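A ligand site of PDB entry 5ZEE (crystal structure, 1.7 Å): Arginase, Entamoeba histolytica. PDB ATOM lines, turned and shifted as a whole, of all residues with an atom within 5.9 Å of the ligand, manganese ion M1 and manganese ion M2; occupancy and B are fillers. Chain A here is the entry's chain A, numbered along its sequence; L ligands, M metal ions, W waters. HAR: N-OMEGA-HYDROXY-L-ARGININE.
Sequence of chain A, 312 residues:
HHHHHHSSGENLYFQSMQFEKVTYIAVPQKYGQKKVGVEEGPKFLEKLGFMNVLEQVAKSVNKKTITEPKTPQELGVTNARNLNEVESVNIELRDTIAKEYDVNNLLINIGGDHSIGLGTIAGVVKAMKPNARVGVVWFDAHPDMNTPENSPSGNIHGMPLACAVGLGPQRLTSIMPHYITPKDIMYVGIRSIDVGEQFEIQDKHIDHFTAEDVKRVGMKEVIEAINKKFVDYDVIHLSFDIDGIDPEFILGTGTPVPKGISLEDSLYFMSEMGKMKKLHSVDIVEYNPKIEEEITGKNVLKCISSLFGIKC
Manganese ion M1 is bound by OH1 of the ligand, OD2 of Asp 140, ND1 of His 114, OD2 of Asp 144 and OD2 of Asp 241.
O of the ligand is in hydrogen-bond range of OG of Ser 153 (2.6 Å). The side-chain hydroxyl (OG1) of Thr 255 sits at hydrogen-bond distance from a nitrogen (NH2) of the ligand. An oxygen (OXT) of the ligand is in hydrogen-bond range of the side-chain amide nitrogen (ND2) of Asn 146, at 3.0 Å. A nitrogen (N) of the ligand is in salt-bridge range of the side-chain carboxylate (OD2) of Asp 194, 3.0 Å away. OE2 of Glu 286 is in salt-bridge range of NH2 of the ligand, at 3.6 Å.
Water W6 lies within hydrogen-bond range of the side-chain hydroxyl (OG) of Ser 151 (2.6 Å), an oxygen (OXT) of the ligand (2.7 Å), the backbone carbonyl oxygen (O) of Asn 155 (2.7 Å) and the side-chain hydroxyl (OG) of Ser 153 (3.5 Å). Water W2 lies within hydrogen-bond range of the backbone carbonyl oxygen of Ser 192 (2.6 Å), the side-chain carboxylate of Glu 197 (2.8 Å) and a nitrogen (N) of the ligand (2.8 Å). Water W3 lies within hydrogen-bond range of the side-chain carboxylate of Glu 197 (2.6 Å), a nitrogen (N) of the ligand (2.9 Å), the side-chain amide nitrogen of Asn 146 (3.1 Å), the backbone carbonyl oxygen of Gly 158 (3.3 Å) and the backbone NH of Asp 144 (3.5 Å). Water W4 lies within hydrogen-bond range of a ring nitrogen (NE2) of His 157, the side-chain amide nitrogen of Asn 155 and an oxygen (O) of the ligand. Water W5 lies within hydrogen-bond range of the side-chain hydroxyl (OG1) of Thr 255 (2.7 Å) and a nitrogen (NH2) of the ligand (3.4 Å). Water W1 lies within hydrogen-bond range of the side-chain carboxylate of Glu 286, a nitrogen (NH2) of the ligand and the side-chain hydroxyl of Thr 255.
NE1 of Trp 138 lies close to OD2 of Asp 140 (3.0 Å). The backbone NH of His 114 is in hydrogen-bond range of the side-chain carboxylate of Glu 286 (2.8 Å). The side-chain carboxylate of Glu 197 is in hydrogen-bond range of the backbone NH of Asp 144 (3.0 Å). The backbone NH (N) of Asp 241 lies within hydrogen-bond range of the backbone carbonyl oxygen (O) of Phe 139, at 2.8 Å. The side-chain hydroxyl of Thr 255 sits close to the side-chain carboxylate of Asp 243 (3.0 Å). The side-chain hydroxyl (OG) of Ser 153 lies within hydrogen-bond range of the backbone NH (N) of Asn 155. The backbone NH (N) of Asn 146 is in hydrogen-bond range of the backbone carbonyl oxygen (O) of Gly 158, 3.1 Å away. A ring nitrogen (ND1) of His 157 sits at hydrogen-bond distance from the side-chain carboxylate of Glu 286, 2.8 Å away.
CD of Pro 152 touches OXT of the ligand (3.8 Å). His 157 touches the ligand. CA of Gly 158 touches CD of the ligand, at 3.6 Å. Within 4 Å of the ligand: His 114, Asp 140, His 142, Asp 144, Asn 146, Pro 152, Ser 153, His 157, Gly 158, Asp 194, Asp 241, Asp 243, Thr 255 and Glu 286. The nearest printed residue that does not touch the ligand is Ser 151 (4.1 Å).
Manganese ion M2 is bound by OH1 of the ligand (1.9 Å), OD2 of Asp 241 (2.3 Å), OD1 of Asp 140 (2.3 Å), OD2 of Asp 243 (2.4 Å), ND1 of His 142 (2.5 Å) and OD1 of Asp 243 (2.5 Å). Manganese ion M2 has six donor atoms within binding distance. Slightly farther from manganese ion M2 lies a nitrogen (NH2) of the ligand (2.8 Å).
Within 4 Å of manganese ion M2: Asp 140, His 142, Asp 241 and Asp 243.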
ATOM      1  N   HIS A 114     -11.452 -20.361 -31.993  1.00  0.00           N
ATOM      2  CA  HIS A 114     -11.753 -21.117 -30.765  1.00  0.00           C
ATOM      3  C   HIS A 114     -13.039 -20.723 -30.071  1.00  0.00           C
ATOM      4  O   HIS A 114     -13.453 -21.415 -29.125  1.00  0.00           O
ATOM      5  CB  HIS A 114     -10.580 -21.124 -29.769  1.00  0.00           C
ATOM      6  CG  HIS A 114     -10.400 -22.434 -29.078  1.00  0.00           C
ATOM      7  ND1 HIS A 114      -9.232 -22.771 -28.434  1.00  0.00           N
ATOM      8  CD2 HIS A 114     -11.203 -23.523 -29.015  1.00  0.00           C
ATOM      9  CE1 HIS A 114      -9.360 -23.997 -27.946  1.00  0.00           C
ATOM     10  NE2 HIS A 114     -10.533 -24.488 -28.313  1.00  0.00           N
ATOM     11  N   TRP A 138      -7.763 -29.014 -22.852  1.00  0.00           N
ATOM     12  CA  TRP A 138      -7.720 -27.779 -23.656  1.00  0.00           C
ATOM     13  C   TRP A 138      -6.268 -27.520 -23.943  1.00  0.00           C
ATOM     14  O   TRP A 138      -5.532 -27.059 -23.084  1.00  0.00           O
ATOM     15  CB  TRP A 138      -8.373 -26.657 -22.868  1.00  0.00           C
ATOM     16  CG  TRP A 138      -8.689 -25.438 -23.588  1.00  0.00           C
ATOM     17  CD1 TRP A 138      -7.898 -24.343 -23.761  1.00  0.00           C
ATOM     18  CD2 TRP A 138      -9.937 -25.114 -24.190  1.00  0.00           C
ATOM     19  NE1 TRP A 138      -8.581 -23.357 -24.462  1.00  0.00           N
ATOM     20  CE2 TRP A 138      -9.840 -23.806 -24.723  1.00  0.00           C
ATOM     21  CE3 TRP A 138     -11.129 -25.806 -24.356  1.00  0.00           C
ATOM     22  CZ2 TRP A 138     -10.925 -23.174 -25.417  1.00  0.00           C
ATOM     23  CZ3 TRP A 138     -12.184 -25.184 -25.039  1.00  0.00           C
ATOM     24  CH2 TRP A 138     -12.068 -23.893 -25.556  1.00  0.00           C
ATOM     25  N   PHE A 139      -5.835 -27.861 -25.146  1.00  0.00           N
ATOM     26  CA  PHE A 139      -4.462 -27.676 -25.583  1.00  0.00           C
ATOM     27  C   PHE A 139      -4.394 -26.345 -26.318  1.00  0.00           C
ATOM     28  O   PHE A 139      -5.052 -26.144 -27.341  1.00  0.00           O
ATOM     29  CB  PHE A 139      -4.112 -28.824 -26.545  1.00  0.00           C
ATOM     30  CG  PHE A 139      -2.718 -28.787 -27.086  1.00  0.00           C
ATOM     31  CD1 PHE A 139      -2.360 -27.977 -28.177  1.00  0.00           C
ATOM     32  CD2 PHE A 139      -1.740 -29.623 -26.534  1.00  0.00           C
ATOM     33  CE1 PHE A 139      -1.061 -27.970 -28.711  1.00  0.00           C
ATOM     34  CE2 PHE A 139      -0.454 -29.618 -27.039  1.00  0.00           C
ATOM     35  CZ  PHE A 139      -0.112 -28.819 -28.141  1.00  0.00           C
ATOM     36  N   ASP A 140      -3.575 -25.431 -25.806  1.00  0.00           N
ATOM     37  CA  ASP A 140      -3.685 -24.034 -26.229  1.00  0.00           C
ATOM     38  C   ASP A 140      -2.573 -23.219 -25.623  1.00  0.00           C
ATOM     39  O   ASP A 140      -2.054 -23.561 -24.548  1.00  0.00           O
ATOM     40  CB  ASP A 140      -5.022 -23.509 -25.691  1.00  0.00           C
ATOM     41  CG  ASP A 140      -5.596 -22.364 -26.520  1.00  0.00           C
ATOM     42  OD1 ASP A 140      -4.868 -21.440 -26.907  1.00  0.00           O
ATOM     43  OD2 ASP A 140      -6.824 -22.420 -26.707  1.00  0.00           O
ATOM     44  N   ALA A 141      -2.131 -22.178 -26.315  1.00  0.00           N
ATOM     45  CA  ALA A 141      -1.328 -21.107 -25.659  1.00  0.00           C
ATOM     46  C   ALA A 141      -2.133 -20.250 -24.638  1.00  0.00           C
ATOM     47  O   ALA A 141      -1.544 -19.646 -23.719  1.00  0.00           O
ATOM     48  CB  ALA A 141      -0.692 -20.231 -26.689  1.00  0.00           C
ATOM     49  N   HIS A 142      -3.467 -20.229 -24.788  1.00  0.00           N
ATOM     50  CA  HIS A 142      -4.340 -19.356 -24.022  1.00  0.00           C
ATOM     51  C   HIS A 142      -5.381 -20.155 -23.219  1.00  0.00           C
ATOM     52  O   HIS A 142      -5.916 -21.126 -23.711  1.00  0.00           O
ATOM     53  CB  HIS A 142      -5.113 -18.436 -24.983  1.00  0.00           C
ATOM     54  CG  HIS A 142      -4.235 -17.732 -25.935  1.00  0.00           C
ATOM     55  ND1 HIS A 142      -3.997 -18.212 -27.204  1.00  0.00           N
ATOM     56  CD2 HIS A 142      -3.508 -16.598 -25.809  1.00  0.00           C
ATOM     57  CE1 HIS A 142      -3.115 -17.409 -27.800  1.00  0.00           C
ATOM     58  NE2 HIS A 142      -2.824 -16.410 -26.978  1.00  0.00           N
ATOM     59  N   ASP A 144      -8.389 -19.021 -22.518  1.00  0.00           N
ATOM     60  CA  ASP A 144      -9.693 -18.710 -23.123  1.00  0.00           C
ATOM     61  C   ASP A 144     -10.785 -18.630 -22.055  1.00  0.00           C
ATOM     62  O   ASP A 144     -11.924 -19.077 -22.250  1.00  0.00           O
ATOM     63  CB  ASP A 144     -10.036 -19.750 -24.204  1.00  0.00           C
ATOM     64  CG  ASP A 144      -9.141 -19.643 -25.443  1.00  0.00           C
ATOM     65  OD1 ASP A 144      -8.471 -18.609 -25.574  1.00  0.00           O
ATOM     66  OD2 ASP A 144      -9.052 -20.615 -26.271  1.00  0.00           O
ATOM     67  N   ASN A 146     -11.525 -15.443 -20.438  1.00  0.00           N
ATOM     68  CA  ASN A 146     -11.821 -14.046 -20.223  1.00  0.00           C
ATOM     69  C   ASN A 146     -13.335 -13.854 -20.340  1.00  0.00           C
ATOM     70  O   ASN A 146     -14.042 -14.719 -20.838  1.00  0.00           O
ATOM     71  CB  ASN A 146     -11.141 -13.204 -21.302  1.00  0.00           C
ATOM     72  CG  ASN A 146      -9.646 -13.035 -21.067  1.00  0.00           C
ATOM     73  OD1 ASN A 146      -9.206 -12.909 -19.935  1.00  0.00           O
ATOM     74  ND2 ASN A 146      -8.896 -12.998 -22.118  1.00  0.00           N
ATOM     75  N   SER A 151     -11.927  -8.663 -20.873  1.00  0.00           N
ATOM     76  CA  SER A 151     -11.240  -9.047 -22.119  1.00  0.00           C
ATOM     77  C   SER A 151     -10.409  -7.899 -22.633  1.00  0.00           C
ATOM     78  O   SER A 151     -10.912  -6.803 -22.710  1.00  0.00           O
ATOM     79  CB  SER A 151     -12.212  -9.441 -23.227  1.00  0.00           C
ATOM     80  OG  SER A 151     -11.490  -9.590 -24.437  1.00  0.00           O
ATOM     81  N   PRO A 152      -9.153  -8.143 -23.028  1.00  0.00           N
ATOM     82  CA  PRO A 152      -8.400  -7.019 -23.624  1.00  0.00           C
ATOM     83  C   PRO A 152      -8.782  -6.682 -25.048  1.00  0.00           C
ATOM     84  O   PRO A 152      -8.381  -5.657 -25.543  1.00  0.00           O
ATOM     85  CB  PRO A 152      -6.938  -7.519 -23.581  1.00  0.00           C
ATOM     86  CG  PRO A 152      -7.070  -9.003 -23.705  1.00  0.00           C
ATOM     87  CD  PRO A 152      -8.341  -9.378 -22.953  1.00  0.00           C
ATOM     88  N   SER A 153      -9.529  -7.545 -25.738  1.00  0.00           N
ATOM     89  CA  SER A 153      -9.808  -7.385 -27.150  1.00  0.00           C
ATOM     90  C   SER A 153     -11.298  -7.342 -27.522  1.00  0.00           C
ATOM     91  O   SER A 153     -11.638  -6.877 -28.603  1.00  0.00           O
ATOM     92  CB  SER A 153      -9.198  -8.608 -27.844  1.00  0.00           C
ATOM     93  OG  SER A 153      -9.835  -9.834 -27.413  1.00  0.00           O
ATOM     94  N   GLY A 154     -12.198  -7.861 -26.685  1.00  0.00           N
ATOM     95  CA  GLY A 154     -13.591  -8.107 -27.098  1.00  0.00           C
ATOM     96  C   GLY A 154     -13.822  -9.306 -28.012  1.00  0.00           C
ATOM     97  O   GLY A 154     -14.946  -9.579 -28.432  1.00  0.00           O
ATOM     98  N   ASN A 155     -12.756 -10.071 -28.283  1.00  0.00           N
ATOM     99  CA  ASN A 155     -12.795 -11.217 -29.198  1.00  0.00           C
ATOM    100  C   ASN A 155     -13.284 -12.454 -28.414  1.00  0.00           C
ATOM    101  O   ASN A 155     -12.669 -12.875 -27.458  1.00  0.00           O
ATOM    102  CB  ASN A 155     -11.436 -11.478 -29.803  1.00  0.00           C
ATOM    103  CG  ASN A 155     -10.993 -10.410 -30.762  1.00  0.00           C
ATOM    104  OD1 ASN A 155     -11.801  -9.653 -31.315  1.00  0.00           O
ATOM    105  ND2 ASN A 155      -9.679 -10.365 -31.000  1.00  0.00           N
ATOM    106  N   HIS A 157     -13.297 -15.504 -29.055  1.00  0.00           N
ATOM    107  CA  HIS A 157     -12.460 -16.698 -29.041  1.00  0.00           C
ATOM    108  C   HIS A 157     -11.599 -16.802 -27.803  1.00  0.00           C
ATOM    109  O   HIS A 157     -11.065 -17.890 -27.514  1.00  0.00           O
ATOM    110  CB  HIS A 157     -11.638 -16.850 -30.353  1.00  0.00           C
ATOM    111  CG  HIS A 157     -10.444 -15.968 -30.473  1.00  0.00           C
ATOM    112  ND1 HIS A 157      -9.405 -16.253 -31.341  1.00  0.00           N
ATOM    113  CD2 HIS A 157     -10.112 -14.822 -29.841  1.00  0.00           C
ATOM    114  CE1 HIS A 157      -8.480 -15.311 -31.218  1.00  0.00           C
ATOM    115  NE2 HIS A 157      -8.873 -14.433 -30.318  1.00  0.00           N
ATOM    116  N   GLY A 158     -11.551 -15.740 -27.021  1.00  0.00           N
ATOM    117  CA  GLY A 158     -10.825 -15.762 -25.781  1.00  0.00           C
ATOM    118  C   GLY A 158     -11.728 -15.972 -24.585  1.00  0.00           C
ATOM    119  O   GLY A 158     -11.295 -15.891 -23.490  1.00  0.00           O
ATOM    120  N   MET A 159     -12.987 -16.304 -24.836  1.00  0.00           N
ATOM    121  CA  MET A 159     -13.973 -16.491 -23.779  1.00  0.00           C
ATOM    122  C   MET A 159     -14.719 -17.821 -23.643  1.00  0.00           C
ATOM    123  O   MET A 159     -15.419 -17.997 -22.701  1.00  0.00           O
ATOM    124  CB  MET A 159     -15.052 -15.420 -23.934  1.00  0.00           C
ATOM    125  CG  MET A 159     -14.576 -13.995 -24.047  1.00  0.00           C
ATOM    126  SD  MET A 159     -15.972 -12.879 -24.307  1.00  0.00           S
ATOM    127  CE  MET A 159     -15.094 -11.476 -24.908  1.00  0.00           C
ATOM    128  N   SER A 192       0.182 -17.670 -22.384  1.00  0.00           N
ATOM    129  CA  SER A 192      -0.202 -16.289 -22.509  1.00  0.00           C
ATOM    130  C   SER A 192      -1.464 -16.162 -21.675  1.00  0.00           C
ATOM    131  O   SER A 192      -2.522 -16.456 -22.119  1.00  0.00           O
ATOM    132  CB  SER A 192      -0.432 -15.902 -23.963  1.00  0.00           C
ATOM    133  OG  SER A 192      -0.958 -14.620 -24.081  1.00  0.00           O
ATOM    134  N   ASP A 194      -3.985 -13.886 -19.068  1.00  0.00           N
ATOM    135  CA  ASP A 194      -4.403 -12.573 -18.631  1.00  0.00           C
ATOM    136  C   ASP A 194      -4.712 -12.534 -17.146  1.00  0.00           C
ATOM    137  O   ASP A 194      -4.809 -13.542 -16.525  1.00  0.00           O
ATOM    138  CB  ASP A 194      -5.616 -12.100 -19.415  1.00  0.00           C
ATOM    139  CG  ASP A 194      -5.320 -11.829 -20.861  1.00  0.00           C
ATOM    140  OD1 ASP A 194      -4.198 -11.451 -21.197  1.00  0.00           O
ATOM    141  OD2 ASP A 194      -6.208 -11.969 -21.675  1.00  0.00           O
ATOM    142  N   GLU A 197      -7.685 -14.648 -15.981  1.00  0.00           N
ATOM    143  CA  GLU A 197      -7.458 -16.052 -16.198  1.00  0.00           C
ATOM    144  C   GLU A 197      -6.540 -16.624 -15.121  1.00  0.00           C
ATOM    145  O   GLU A 197      -6.787 -17.689 -14.605  1.00  0.00           O
ATOM    146  CB  GLU A 197      -6.898 -16.301 -17.581  1.00  0.00           C
ATOM    147  CG  GLU A 197      -7.845 -15.797 -18.696  1.00  0.00           C
ATOM    148  CD  GLU A 197      -7.219 -15.943 -20.068  1.00  0.00           C
ATOM    149  OE1 GLU A 197      -6.054 -15.428 -20.276  1.00  0.00           O
ATOM    150  OE2 GLU A 197      -7.888 -16.565 -20.932  1.00  0.00           O
ATOM    151  N   ASP A 241      -6.199 -26.245 -29.937  1.00  0.00           N
ATOM    152  CA  ASP A 241      -5.814 -25.027 -30.582  1.00  0.00           C
ATOM    153  C   ASP A 241      -4.386 -25.168 -31.051  1.00  0.00           C
ATOM    154  O   ASP A 241      -3.452 -25.385 -30.271  1.00  0.00           O
ATOM    155  CB  ASP A 241      -5.956 -23.878 -29.565  1.00  0.00           C
ATOM    156  CG  ASP A 241      -5.842 -22.491 -30.184  1.00  0.00           C
ATOM    157  OD1 ASP A 241      -5.094 -22.323 -31.189  1.00  0.00           O
ATOM    158  OD2 ASP A 241      -6.464 -21.552 -29.602  1.00  0.00           O
ATOM    159  N   ASP A 243      -2.269 -23.113 -31.896  1.00  0.00           N
ATOM    160  CA  ASP A 243      -1.280 -22.155 -31.350  1.00  0.00           C
ATOM    161  C   ASP A 243      -0.655 -22.600 -30.006  1.00  0.00           C
ATOM    162  O   ASP A 243       0.255 -21.969 -29.503  1.00  0.00           O
ATOM    163  CB  ASP A 243      -1.803 -20.733 -31.307  1.00  0.00           C
ATOM    164  CG  ASP A 243      -2.833 -20.450 -30.231  1.00  0.00           C
ATOM    165  OD1 ASP A 243      -2.967 -21.171 -29.197  1.00  0.00           O
ATOM    166  OD2 ASP A 243      -3.553 -19.426 -30.463  1.00  0.00           O
ATOM    167  N   GLY A 244      -1.155 -23.691 -29.464  1.00  0.00           N
ATOM    168  CA  GLY A 244      -0.408 -24.411 -28.396  1.00  0.00           C
ATOM    169  C   GLY A 244       0.994 -24.779 -28.830  1.00  0.00           C
ATOM    170  O   GLY A 244       1.950 -24.800 -28.020  1.00  0.00           O
ATOM    171  N   THR A 255      -2.962 -15.771 -33.388  1.00  0.00           N
ATOM    172  CA  THR A 255      -2.340 -15.314 -32.160  1.00  0.00           C
ATOM    173  C   THR A 255      -1.199 -16.264 -31.748  1.00  0.00           C
ATOM    174  O   THR A 255      -1.312 -16.956 -30.727  1.00  0.00           O
ATOM    175  CB  THR A 255      -3.374 -15.230 -31.025  1.00  0.00           C
ATOM    176  OG1 THR A 255      -4.034 -16.497 -30.869  1.00  0.00           O
ATOM    177  CG2 THR A 255      -4.465 -14.148 -31.341  1.00  0.00           C
ATOM    178  N   VAL A 285      -8.661 -26.307 -34.031  1.00  0.00           N
ATOM    179  CA  VAL A 285      -9.022 -24.917 -34.265  1.00  0.00           C
ATOM    180  C   VAL A 285      -7.842 -23.996 -34.513  1.00  0.00           C
ATOM    181  O   VAL A 285      -6.704 -24.288 -34.175  1.00  0.00           O
ATOM    182  CB  VAL A 285      -9.847 -24.351 -33.096  1.00  0.00           C
ATOM    183  CG1 VAL A 285     -11.143 -25.144 -32.876  1.00  0.00           C
ATOM    184  CG2 VAL A 285      -9.043 -24.228 -31.815  1.00  0.00           C
ATOM    185  N   GLU A 286      -8.174 -22.860 -35.134  1.00  0.00           N
ATOM    186  CA  GLU A 286      -7.325 -21.702 -35.309  1.00  0.00           C
ATOM    187  C   GLU A 286      -6.325 -21.785 -36.458  1.00  0.00           C
ATOM    188  O   GLU A 286      -5.433 -20.965 -36.533  1.00  0.00           O
ATOM    189  CB  GLU A 286      -6.669 -21.237 -33.983  1.00  0.00           C
ATOM    190  CG  GLU A 286      -7.634 -20.779 -32.893  1.00  0.00           C
ATOM    191  CD  GLU A 286      -8.248 -19.346 -33.121  1.00  0.00           C
ATOM    192  OE1 GLU A 286      -7.910 -18.642 -34.113  1.00  0.00           O
ATOM    193  OE2 GLU A 286      -9.038 -18.877 -32.240  1.00  0.00           O
HETATM  194  N   HAR L   1      -6.267 -13.461 -24.270  1.00  0.00           N
HETATM  195  CA  HAR L   1      -6.438 -12.911 -25.663  1.00  0.00           C
HETATM  196  C   HAR L   1      -7.796 -12.201 -25.831  1.00  0.00           C
HETATM  197  O   HAR L   1      -7.811 -11.332 -26.744  1.00  0.00           O
HETATM  198  CB  HAR L   1      -6.300 -14.014 -26.702  1.00  0.00           C
HETATM  199  CG  HAR L   1      -7.188 -15.220 -26.310  1.00  0.00           C
HETATM  200  CD  HAR L   1      -7.640 -16.151 -27.412  1.00  0.00           C
HETATM  201  NE  HAR L   1      -6.771 -16.660 -28.241  1.00  0.00           N
HETATM  202  CZ  HAR L   1      -7.239 -17.611 -29.252  1.00  0.00           C
HETATM  203  NH1 HAR L   1      -7.755 -18.803 -28.520  1.00  0.00           N
HETATM  204  NH2 HAR L   1      -6.198 -17.850 -30.224  1.00  0.00           N
HETATM  205  OH1 HAR L   1      -6.890 -19.797 -28.020  1.00  0.00           O
HETATM  206  OXT HAR L   1      -8.759 -12.532 -25.042  1.00  0.00           O
HETATM  207 MN    MN M   1      -7.948 -21.378 -27.910  1.00  0.00          MN
HETATM  208 MN    MN M   2      -5.099 -19.895 -28.661  1.00  0.00          MN
HETATM  209  O   HOH W   1      -6.390 -16.630 -33.390  1.00  0.00           O
HETATM  210  O   HOH W   2      -4.833 -15.367 -22.749  1.00  0.00           O
HETATM  211  O   HOH W   3      -7.975 -15.685 -23.373  1.00  0.00           O
HETATM  212  O   HOH W   4      -7.666 -12.092 -29.834  1.00  0.00           O
HETATM  213  O   HOH W   5      -4.241 -18.313 -32.907  1.00  0.00           O
HETATM  214  O   HOH W   6     -11.358 -12.017 -25.212  1.00  0.00           O
